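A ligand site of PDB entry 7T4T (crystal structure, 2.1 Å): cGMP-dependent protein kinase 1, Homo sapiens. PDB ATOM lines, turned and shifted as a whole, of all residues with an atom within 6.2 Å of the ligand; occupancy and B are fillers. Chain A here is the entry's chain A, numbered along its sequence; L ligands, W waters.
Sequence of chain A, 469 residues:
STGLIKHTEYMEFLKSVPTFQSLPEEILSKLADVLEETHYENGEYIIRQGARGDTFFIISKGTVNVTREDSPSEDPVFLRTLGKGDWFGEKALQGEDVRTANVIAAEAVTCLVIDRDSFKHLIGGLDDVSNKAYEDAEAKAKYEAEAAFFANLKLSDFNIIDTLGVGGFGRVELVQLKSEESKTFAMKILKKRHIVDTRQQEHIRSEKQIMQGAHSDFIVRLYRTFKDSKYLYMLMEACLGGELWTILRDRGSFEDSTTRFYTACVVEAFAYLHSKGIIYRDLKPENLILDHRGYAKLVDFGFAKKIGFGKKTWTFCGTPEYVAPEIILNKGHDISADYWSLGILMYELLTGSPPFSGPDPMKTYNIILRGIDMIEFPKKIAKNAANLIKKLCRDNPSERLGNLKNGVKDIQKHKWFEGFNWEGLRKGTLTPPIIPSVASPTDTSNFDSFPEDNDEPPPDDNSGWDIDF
The backbone carbonyl oxygen (O) of Glu 237 sits at hydrogen-bond distance from a nitrogen (N3) of the ligand (2.7 Å).
O13 of the ligand is in hydrogen-bond range of OE2 of Glu 243, at 2.9 Å.
An oxygen (O1) of the ligand lies within hydrogen-bond range of the backbone NH (N) of Gly 168 (3.0 Å).
N of Cys 239 sits at hydrogen-bond distance from N4 of the ligand (3.2 Å).
NZ of Lys 188 is in salt-bridge range of O7 of the ligand, at 3.7 Å.
The backbone NH (N) of Glu 237 lies within hydrogen-bond range of the backbone carbonyl oxygen (O) of Arg 221.
NE1 of Trp 245 lies within hydrogen-bond range of OE1 of Glu 243 (2.8 Å).
The backbone carbonyl oxygen (O) of Ala 186 lies within hydrogen-bond range of the backbone NH (N) of Met 236 (2.8 Å).
O of Asn 287 lies within hydrogen-bond range of N of Val 299, 3.1 Å away.
The backbone NH (N) of Val 172 lies within hydrogen-bond range of the backbone carbonyl oxygen (O) of Gly 165, 2.7 Å away.
The backbone carbonyl oxygen (O) of Val 172 lies within hydrogen-bond range of the backbone NH (N) of Leu 164 (2.7 Å).
The backbone carbonyl oxygen of Gly 170 sits close to an oxygen (O8) of the ligand (3.4 Å).
CD1 of Leu 164 touches C9 of the ligand, at 3.7 Å.
C of Gly 165 touches C1 of the ligand (3.7 Å).
Val 166 touches the ligand (N to C1, 3.9 Å).
Gly 167 touches the ligand (CA to O5, 3.2 Å).
Val 172 touches the ligand.
Ala 186 touches the ligand.
Val 220 touches the ligand (CG1 to N3, 3.5 Å).
CE of Met 236 touches N2 of the ligand, 3.9 Å away.
Ala 238 touches the ligand.
Ile 289 touches the ligand (CD1 to N5, 3.3 Å).
CG2 of Val 299 touches N2 of the ligand, 3.5 Å away.
OD2 of Asp 300 touches O6 of the ligand (3.8 Å).
Phe 447 touches the ligand.
Hydrophobic or aromatic side chains that line the ligand: Leu 164, Val 172, Ala 186, Val 220, Met 236, Ile 289, Val 299 and Phe 447.
Along chain A the residues within 4 Å of the ligand span positions 164 to 447.
Water W1 lies within hydrogen-bond range of the side-chain amide oxygen (OD1) of Asn 287 (2.6 Å), the side-chain carboxylate (OD2) of Asp 300 (2.7 Å) and an oxygen (O4) of the ligand (2.7 Å).
Water W2 bridges O3 of the ligand (3.0 Å) and OD2 of Asp 300 (3.1 Å).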
ATOM      1  N   LEU A 164     -14.632  15.951  -6.329  1.00  0.00           N
ATOM      2  CA  LEU A 164     -13.944  17.220  -6.469  1.00  0.00           C
ATOM      3  C   LEU A 164     -14.402  17.872  -7.738  1.00  0.00           C
ATOM      4  O   LEU A 164     -14.667  19.074  -7.742  1.00  0.00           O
ATOM      5  CB  LEU A 164     -12.416  17.035  -6.443  1.00  0.00           C
ATOM      6  CG  LEU A 164     -11.861  16.677  -5.065  1.00  0.00           C
ATOM      7  CD1 LEU A 164     -10.497  15.995  -5.176  1.00  0.00           C
ATOM      8  CD2 LEU A 164     -11.787  17.895  -4.182  1.00  0.00           C
ATOM      9  N   GLY A 165     -14.485  17.110  -8.812  1.00  0.00           N
ATOM     10  CA  GLY A 165     -14.941  17.635 -10.094  1.00  0.00           C
ATOM     11  C   GLY A 165     -15.048  16.596 -11.182  1.00  0.00           C
ATOM     12  O   GLY A 165     -14.525  15.481 -11.049  1.00  0.00           O
ATOM     13  N   VAL A 166     -15.752  16.947 -12.253  1.00  0.00           N
ATOM     14  CA  VAL A 166     -15.941  16.070 -13.419  1.00  0.00           C
ATOM     15  C   VAL A 166     -15.496  16.820 -14.664  1.00  0.00           C
ATOM     16  O   VAL A 166     -16.038  17.892 -14.966  1.00  0.00           O
ATOM     17  CB  VAL A 166     -17.386  15.534 -13.547  1.00  0.00           C
ATOM     18  CG1 VAL A 166     -17.500  14.568 -14.730  1.00  0.00           C
ATOM     19  CG2 VAL A 166     -17.829  14.849 -12.253  1.00  0.00           C
ATOM     20  N   GLY A 167     -14.505  16.257 -15.359  1.00  0.00           N
ATOM     21  CA  GLY A 167     -13.981  16.797 -16.602  1.00  0.00           C
ATOM     22  C   GLY A 167     -14.595  16.097 -17.800  1.00  0.00           C
ATOM     23  O   GLY A 167     -15.488  15.250 -17.639  1.00  0.00           O
ATOM     24  N   GLY A 168     -14.105  16.446 -18.982  1.00  0.00           N
ATOM     25  CA  GLY A 168     -14.587  15.898 -20.242  1.00  0.00           C
ATOM     26  C   GLY A 168     -14.355  14.412 -20.432  1.00  0.00           C
ATOM     27  O   GLY A 168     -15.113  13.771 -21.170  1.00  0.00           O
ATOM     28  N   PHE A 169     -13.291  13.850 -19.800  1.00  0.00           N
ATOM     29  CA  PHE A 169     -12.948  12.429 -19.952  1.00  0.00           C
ATOM     30  C   PHE A 169     -12.785  11.663 -18.615  1.00  0.00           C
ATOM     31  O   PHE A 169     -12.229  10.565 -18.640  1.00  0.00           O
ATOM     32  CB  PHE A 169     -11.678  12.283 -20.822  1.00  0.00           C
ATOM     33  CG  PHE A 169     -11.604  13.221 -22.009  1.00  0.00           C
ATOM     34  CD1 PHE A 169     -10.940  14.440 -21.925  1.00  0.00           C
ATOM     35  CD2 PHE A 169     -12.221  12.896 -23.222  1.00  0.00           C
ATOM     36  CE1 PHE A 169     -10.884  15.316 -23.015  1.00  0.00           C
ATOM     37  CE2 PHE A 169     -12.156  13.775 -24.311  1.00  0.00           C
ATOM     38  CZ  PHE A 169     -11.491  14.977 -24.200  1.00  0.00           C
ATOM     39  N   GLY A 170     -13.310  12.199 -17.490  1.00  0.00           N
ATOM     40  CA  GLY A 170     -13.235  11.500 -16.205  1.00  0.00           C
ATOM     41  C   GLY A 170     -13.571  12.304 -14.950  1.00  0.00           C
ATOM     42  O   GLY A 170     -13.422  13.536 -14.940  1.00  0.00           O
ATOM     43  N   ARG A 171     -13.945  11.586 -13.867  1.00  0.00           N
ATOM     44  CA  ARG A 171     -14.288  12.192 -12.572  1.00  0.00           C
ATOM     45  C   ARG A 171     -13.137  12.155 -11.532  1.00  0.00           C
ATOM     46  O   ARG A 171     -12.461  11.146 -11.378  1.00  0.00           O
ATOM     47  CB  ARG A 171     -15.584  11.568 -11.993  1.00  0.00           C
ATOM     48  CG  ARG A 171     -15.464  10.150 -11.437  1.00  0.00           C
ATOM     49  CD  ARG A 171     -16.829   9.550 -11.117  1.00  0.00           C
ATOM     50  NE  ARG A 171     -16.716   8.599 -10.000  1.00  0.00           N
ATOM     51  CZ  ARG A 171     -16.427   7.308 -10.091  1.00  0.00           C
ATOM     52  NH1 ARG A 171     -16.252   6.734 -11.278  1.00  0.00           N
ATOM     53  NH2 ARG A 171     -16.316   6.565  -8.981  1.00  0.00           N
ATOM     54  N   VAL A 172     -12.958  13.260 -10.795  1.00  0.00           N
ATOM     55  CA  VAL A 172     -11.941  13.369  -9.750  1.00  0.00           C
ATOM     56  C   VAL A 172     -12.657  13.288  -8.391  1.00  0.00           C
ATOM     57  O   VAL A 172     -13.459  14.143  -8.037  1.00  0.00           O
ATOM     58  CB  VAL A 172     -11.054  14.632  -9.924  1.00  0.00           C
ATOM     59  CG1 VAL A 172     -10.014  14.734  -8.816  1.00  0.00           C
ATOM     60  CG2 VAL A 172     -10.349  14.589 -11.285  1.00  0.00           C
ATOM     61  N   ALA A 186      -6.769  13.097  -4.120  1.00  0.00           N
ATOM     62  CA  ALA A 186      -7.634  13.330  -5.268  1.00  0.00           C
ATOM     63  C   ALA A 186      -7.389  12.126  -6.170  1.00  0.00           C
ATOM     64  O   ALA A 186      -6.238  11.890  -6.566  1.00  0.00           O
ATOM     65  CB  ALA A 186      -7.233  14.620  -5.998  1.00  0.00           C
ATOM     66  N   LYS A 188      -8.239  10.583  -9.777  1.00  0.00           N
ATOM     67  CA  LYS A 188      -8.826  10.789 -11.115  1.00  0.00           C
ATOM     68  C   LYS A 188      -9.109   9.390 -11.691  1.00  0.00           C
ATOM     69  O   LYS A 188      -8.196   8.566 -11.767  1.00  0.00           O
ATOM     70  CB  LYS A 188      -7.890  11.589 -12.032  1.00  0.00           C
ATOM     71  CG  LYS A 188      -8.459  11.951 -13.400  1.00  0.00           C
ATOM     72  CD  LYS A 188      -7.371  12.590 -14.274  1.00  0.00           C
ATOM     73  CE  LYS A 188      -7.756  13.886 -14.918  1.00  0.00           C
ATOM     74  NZ  LYS A 188      -6.577  14.553 -15.579  1.00  0.00           N
ATOM     75  N   LEU A 190     -10.543   7.402 -14.970  1.00  0.00           N
ATOM     76  CA  LEU A 190     -10.779   7.533 -16.411  1.00  0.00           C
ATOM     77  C   LEU A 190     -11.275   6.206 -16.935  1.00  0.00           C
ATOM     78  O   LEU A 190     -10.725   5.163 -16.552  1.00  0.00           O
ATOM     79  CB  LEU A 190      -9.469   7.901 -17.130  1.00  0.00           C
ATOM     80  CG  LEU A 190      -8.711   9.101 -16.585  1.00  0.00           C
ATOM     81  CD1 LEU A 190      -7.214   8.951 -16.802  1.00  0.00           C
ATOM     82  CD2 LEU A 190      -9.216  10.390 -17.200  1.00  0.00           C
ATOM     83  N   VAL A 220       1.135  19.717  -8.797  1.00  0.00           N
ATOM     84  CA  VAL A 220       0.331  18.701  -8.102  1.00  0.00           C
ATOM     85  C   VAL A 220       1.017  17.312  -8.266  1.00  0.00           C
ATOM     86  O   VAL A 220       1.398  16.949  -9.378  1.00  0.00           O
ATOM     87  CB  VAL A 220      -1.130  18.720  -8.623  1.00  0.00           C
ATOM     88  CG1 VAL A 220      -1.923  17.514  -8.124  1.00  0.00           C
ATOM     89  CG2 VAL A 220      -1.834  20.021  -8.203  1.00  0.00           C
ATOM     90  N   ARG A 221       1.239  16.590  -7.161  1.00  0.00           N
ATOM     91  CA  ARG A 221       1.902  15.292  -7.241  1.00  0.00           C
ATOM     92  C   ARG A 221       0.949  14.206  -7.742  1.00  0.00           C
ATOM     93  O   ARG A 221      -0.224  14.202  -7.381  1.00  0.00           O
ATOM     94  CB  ARG A 221       2.474  14.853  -5.863  1.00  0.00           C
ATOM     95  CG  ARG A 221       3.823  15.512  -5.482  1.00  0.00           C
ATOM     96  CD  ARG A 221       5.042  14.973  -6.243  1.00  0.00           C
ATOM     97  NE  ARG A 221       5.160  13.511  -6.198  1.00  0.00           N
ATOM     98  CZ  ARG A 221       5.032  12.667  -7.225  1.00  0.00           C
ATOM     99  NH1 ARG A 221       4.780  13.125  -8.455  1.00  0.00           N
ATOM    100  NH2 ARG A 221       5.162  11.351  -7.035  1.00  0.00           N
ATOM    101  N   MET A 236      -3.550  11.332  -6.796  1.00  0.00           N
ATOM    102  CA  MET A 236      -2.886  12.616  -6.715  1.00  0.00           C
ATOM    103  C   MET A 236      -3.031  13.304  -5.359  1.00  0.00           C
ATOM    104  O   MET A 236      -3.904  12.990  -4.555  1.00  0.00           O
ATOM    105  CB  MET A 236      -3.466  13.584  -7.755  1.00  0.00           C
ATOM    106  CG  MET A 236      -3.320  13.135  -9.192  1.00  0.00           C
ATOM    107  SD  MET A 236      -4.119  14.323 -10.307  1.00  0.00           S
ATOM    108  CE  MET A 236      -5.877  13.964  -9.959  1.00  0.00           C
ATOM    109  N   GLU A 237      -2.215  14.324  -5.169  1.00  0.00           N
ATOM    110  CA  GLU A 237      -2.268  15.240  -4.035  1.00  0.00           C
ATOM    111  C   GLU A 237      -3.615  16.001  -4.098  1.00  0.00           C
ATOM    112  O   GLU A 237      -3.937  16.545  -5.156  1.00  0.00           O
ATOM    113  CB  GLU A 237      -1.099  16.203  -4.161  1.00  0.00           C
ATOM    114  CG  GLU A 237      -1.079  17.421  -3.272  1.00  0.00           C
ATOM    115  CD  GLU A 237       0.095  18.325  -3.558  1.00  0.00           C
ATOM    116  OE1 GLU A 237       0.902  18.018  -4.472  1.00  0.00           O
ATOM    117  OE2 GLU A 237       0.206  19.373  -2.873  1.00  0.00           O
ATOM    118  N   ALA A 238      -4.373  16.051  -2.989  1.00  0.00           N
ATOM    119  CA  ALA A 238      -5.643  16.803  -2.934  1.00  0.00           C
ATOM    120  C   ALA A 238      -5.316  18.247  -2.570  1.00  0.00           C
ATOM    121  O   ALA A 238      -4.719  18.493  -1.516  1.00  0.00           O
ATOM    122  CB  ALA A 238      -6.581  16.202  -1.891  1.00  0.00           C
ATOM    123  N   CYS A 239      -5.710  19.196  -3.422  1.00  0.00           N
ATOM    124  CA  CYS A 239      -5.497  20.628  -3.238  1.00  0.00           C
ATOM    125  C   CYS A 239      -6.878  21.209  -2.958  1.00  0.00           C
ATOM    126  O   CYS A 239      -7.636  21.452  -3.886  1.00  0.00           O
ATOM    127  CB  CYS A 239      -4.857  21.212  -4.489  1.00  0.00           C
ATOM    128  SG  CYS A 239      -3.149  20.672  -4.760  1.00  0.00           S
ATOM    129  N   LEU A 240      -7.220  21.393  -1.672  1.00  0.00           N
ATOM    130  CA  LEU A 240      -8.560  21.786  -1.220  1.00  0.00           C
ATOM    131  C   LEU A 240      -8.841  23.293  -1.154  1.00  0.00           C
ATOM    132  O   LEU A 240      -9.965  23.657  -0.846  1.00  0.00           O
ATOM    133  CB  LEU A 240      -8.877  21.131   0.146  1.00  0.00           C
ATOM    134  CG  LEU A 240      -8.754  19.596   0.183  1.00  0.00           C
ATOM    135  CD1 LEU A 240      -9.006  19.071   1.609  1.00  0.00           C
ATOM    136  CD2 LEU A 240      -9.736  18.948  -0.786  1.00  0.00           C
ATOM    137  N   GLU A 243      -9.884  25.995  -7.299  1.00  0.00           N
ATOM    138  CA  GLU A 243      -9.293  26.332  -8.600  1.00  0.00           C
ATOM    139  C   GLU A 243      -9.113  27.863  -8.653  1.00  0.00           C
ATOM    140  O   GLU A 243     -10.030  28.587  -8.251  1.00  0.00           O
ATOM    141  CB  GLU A 243     -10.240  25.902  -9.746  1.00  0.00           C
ATOM    142  CG  GLU A 243     -10.675  24.449  -9.727  1.00  0.00           C
ATOM    143  CD  GLU A 243     -11.916  24.200 -10.570  1.00  0.00           C
ATOM    144  OE1 GLU A 243     -11.817  24.309 -11.810  1.00  0.00           O
ATOM    145  OE2 GLU A 243     -12.978  23.868  -9.986  1.00  0.00           O
ATOM    146  N   TRP A 245      -9.349  29.821 -11.236  1.00  0.00           N
ATOM    147  CA  TRP A 245     -10.351  30.438 -12.138  1.00  0.00           C
ATOM    148  C   TRP A 245     -11.677  30.820 -11.386  1.00  0.00           C
ATOM    149  O   TRP A 245     -12.221  31.900 -11.635  1.00  0.00           O
ATOM    150  CB  TRP A 245     -10.632  29.572 -13.403  1.00  0.00           C
ATOM    151  CG  TRP A 245     -11.743  28.566 -13.284  1.00  0.00           C
ATOM    152  CD1 TRP A 245     -11.635  27.254 -12.918  1.00  0.00           C
ATOM    153  CD2 TRP A 245     -13.139  28.802 -13.554  1.00  0.00           C
ATOM    154  NE1 TRP A 245     -12.877  26.646 -12.975  1.00  0.00           N
ATOM    155  CE2 TRP A 245     -13.819  27.589 -13.316  1.00  0.00           C
ATOM    156  CE3 TRP A 245     -13.881  29.923 -13.965  1.00  0.00           C
ATOM    157  CZ2 TRP A 245     -15.207  27.469 -13.452  1.00  0.00           C
ATOM    158  CZ3 TRP A 245     -15.249  29.812 -14.108  1.00  0.00           C
ATOM    159  CH2 TRP A 245     -15.904  28.601 -13.836  1.00  0.00           C
ATOM    160  N   LYS A 284      -3.238  28.416 -17.878  1.00  0.00           N
ATOM    161  CA  LYS A 284      -4.478  29.198 -17.864  1.00  0.00           C
ATOM    162  C   LYS A 284      -4.955  29.185 -16.414  1.00  0.00           C
ATOM    163  O   LYS A 284      -4.545  28.279 -15.674  1.00  0.00           O
ATOM    164  CB  LYS A 284      -5.544  28.636 -18.817  1.00  0.00           C
ATOM    165  CG  LYS A 284      -5.758  27.147 -18.714  1.00  0.00           C
ATOM    166  CD  LYS A 284      -6.831  26.696 -19.649  1.00  0.00           C
ATOM    167  CE  LYS A 284      -7.048  25.203 -19.579  1.00  0.00           C
ATOM    168  NZ  LYS A 284      -8.094  24.731 -20.516  1.00  0.00           N
ATOM    169  N   GLU A 286      -7.634  28.062 -15.002  1.00  0.00           N
ATOM    170  CA  GLU A 286      -8.281  26.793 -14.610  1.00  0.00           C
ATOM    171  C   GLU A 286      -7.296  25.653 -14.390  1.00  0.00           C
ATOM    172  O   GLU A 286      -7.709  24.632 -13.848  1.00  0.00           O
ATOM    173  CB  GLU A 286      -9.439  26.329 -15.524  1.00  0.00           C
ATOM    174  CG  GLU A 286      -9.332  26.635 -16.991  1.00  0.00           C
ATOM    175  CD  GLU A 286      -9.786  28.043 -17.331  1.00  0.00           C
ATOM    176  OE1 GLU A 286     -10.994  28.241 -17.563  1.00  0.00           O
ATOM    177  OE2 GLU A 286      -8.934  28.955 -17.322  1.00  0.00           O
ATOM    178  N   ASN A 287      -6.007  25.818 -14.739  1.00  0.00           N
ATOM    179  CA  ASN A 287      -4.982  24.811 -14.510  1.00  0.00           C
ATOM    180  C   ASN A 287      -4.097  25.142 -13.314  1.00  0.00           C
ATOM    181  O   ASN A 287      -3.062  24.519 -13.127  1.00  0.00           O
ATOM    182  CB  ASN A 287      -4.171  24.610 -15.821  1.00  0.00           C
ATOM    183  CG  ASN A 287      -4.882  23.673 -16.759  1.00  0.00           C
ATOM    184  OD1 ASN A 287      -5.892  23.076 -16.459  1.00  0.00           O
ATOM    185  ND2 ASN A 287      -4.371  23.488 -17.916  1.00  0.00           N
ATOM    186  N   ILE A 289      -4.335  25.414  -9.168  1.00  0.00           N
ATOM    187  CA  ILE A 289      -5.207  24.980  -8.085  1.00  0.00           C
ATOM    188  C   ILE A 289      -4.537  25.361  -6.790  1.00  0.00           C
ATOM    189  O   ILE A 289      -3.326  25.262  -6.697  1.00  0.00           O
ATOM    190  CB  ILE A 289      -5.481  23.450  -8.228  1.00  0.00           C
ATOM    191  CG1 ILE A 289      -6.642  23.004  -7.361  1.00  0.00           C
ATOM    192  CG2 ILE A 289      -4.230  22.614  -7.903  1.00  0.00           C
ATOM    193  CD1 ILE A 289      -7.154  21.678  -7.678  1.00  0.00           C
ATOM    194  N   VAL A 299      -1.822  21.778 -12.471  1.00  0.00           N
ATOM    195  CA  VAL A 299      -2.523  20.494 -12.285  1.00  0.00           C
ATOM    196  C   VAL A 299      -2.776  19.656 -13.581  1.00  0.00           C
ATOM    197  O   VAL A 299      -2.888  18.426 -13.442  1.00  0.00           O
ATOM    198  CB  VAL A 299      -3.849  20.724 -11.491  1.00  0.00           C
ATOM    199  CG1 VAL A 299      -4.930  21.383 -12.326  1.00  0.00           C
ATOM    200  CG2 VAL A 299      -4.352  19.428 -10.896  1.00  0.00           C
ATOM    201  N   ASP A 300      -2.917  20.242 -14.767  1.00  0.00           N
ATOM    202  CA  ASP A 300      -3.263  19.431 -15.950  1.00  0.00           C
ATOM    203  C   ASP A 300      -2.065  19.290 -16.909  1.00  0.00           C
ATOM    204  O   ASP A 300      -1.613  20.296 -17.462  1.00  0.00           O
ATOM    205  CB  ASP A 300      -4.496  20.057 -16.652  1.00  0.00           C
ATOM    206  CG  ASP A 300      -5.246  19.208 -17.654  1.00  0.00           C
ATOM    207  OD1 ASP A 300      -4.603  18.340 -18.295  1.00  0.00           O
ATOM    208  OD2 ASP A 300      -6.459  19.423 -17.830  1.00  0.00           O
ATOM    209  N   PHE A 447     -15.005  23.844  -4.179  1.00  0.00           N
ATOM    210  CA  PHE A 447     -15.277  23.366  -5.548  1.00  0.00           C
ATOM    211  C   PHE A 447     -16.817  23.413  -5.798  1.00  0.00           C
ATOM    212  O   PHE A 447     -17.594  23.076  -4.888  1.00  0.00           O
ATOM    213  CB  PHE A 447     -14.747  21.949  -5.744  1.00  0.00           C
ATOM    214  CG  PHE A 447     -13.256  21.870  -5.579  1.00  0.00           C
ATOM    215  CD1 PHE A 447     -12.693  21.688  -4.330  1.00  0.00           C
ATOM    216  CD2 PHE A 447     -12.415  22.044  -6.672  1.00  0.00           C
ATOM    217  CE1 PHE A 447     -11.310  21.679  -4.166  1.00  0.00           C
ATOM    218  CE2 PHE A 447     -11.035  22.014  -6.514  1.00  0.00           C
ATOM    219  CZ  PHE A 447     -10.485  21.835  -5.255  1.00  0.00           C
HETATM  220  P1  LIG L   1     -10.852  19.037 -19.420  1.00  0.00           P
HETATM  221  O1  LIG L   1     -12.343  18.829 -19.298  1.00  0.00           O
HETATM  222  O2  LIG L   1     -10.459  20.181 -20.377  1.00  0.00           O
HETATM  223  O3  LIG L   1     -10.100  17.756 -19.850  1.00  0.00           O
HETATM  224  P2  LIG L   1     -10.691  19.406 -16.501  1.00  0.00           P
HETATM  225  O4  LIG L   1     -10.044  20.429 -15.660  1.00  0.00           O
HETATM  226  O5  LIG L   1     -12.227  19.454 -16.471  1.00  0.00           O
HETATM  227  O6  LIG L   1     -10.224  19.486 -18.017  1.00  0.00           O
HETATM  228  P3  LIG L   1     -10.200  17.143 -14.735  1.00  0.00           P
HETATM  229  O7  LIG L   1      -8.818  17.186 -14.183  1.00  0.00           O
HETATM  230  O8  LIG L   1     -10.890  15.780 -14.943  1.00  0.00           O
HETATM  231  O9  LIG L   1     -10.260  17.916 -16.123  1.00  0.00           O
HETATM  232  O10 LIG L   1     -11.242  18.067 -13.937  1.00  0.00           O
HETATM  233  C1  LIG L   1     -11.932  17.757 -12.721  1.00  0.00           C
HETATM  234  C2  LIG L   1     -11.737  18.856 -11.703  1.00  0.00           C
HETATM  235  O11 LIG L   1     -11.313  18.282 -10.447  1.00  0.00           O
HETATM  236  C3  LIG L   1     -10.690  19.921 -11.989  1.00  0.00           C
HETATM  237  O12 LIG L   1     -11.128  20.915 -12.916  1.00  0.00           O
HETATM  238  C4  LIG L   1     -10.465  20.495 -10.589  1.00  0.00           C
HETATM  239  O13 LIG L   1     -11.563  21.316 -10.188  1.00  0.00           O
HETATM  240  C5  LIG L   1     -10.518  19.218  -9.740  1.00  0.00           C
HETATM  241  N1  LIG L   1      -9.202  18.632  -9.456  1.00  0.00           N
HETATM  242  C6  LIG L   1      -8.332  18.063 -10.362  1.00  0.00           C
HETATM  243  N2  LIG L   1      -7.213  17.639  -9.813  1.00  0.00           N
HETATM  244  C7  LIG L   1      -7.361  17.945  -8.467  1.00  0.00           C
HETATM  245  C8  LIG L   1      -6.511  17.780  -7.354  1.00  0.00           C
HETATM  246  N3  LIG L   1      -5.314  17.191  -7.424  1.00  0.00           N
HETATM  247  N4  LIG L   1      -6.961  18.205  -6.148  1.00  0.00           N
HETATM  248  C9  LIG L   1      -8.171  18.767  -6.075  1.00  0.00           C
HETATM  249  N5  LIG L   1      -9.045  19.002  -7.058  1.00  0.00           N
HETATM  250  C10 LIG L   1      -8.586  18.563  -8.235  1.00  0.00           C
HETATM  251  O   HOH W   1      -7.912  21.479 -16.923  1.00  0.00           O
HETATM  252  O   HOH W   2      -8.060  16.784 -17.890  1.00  0.00           O
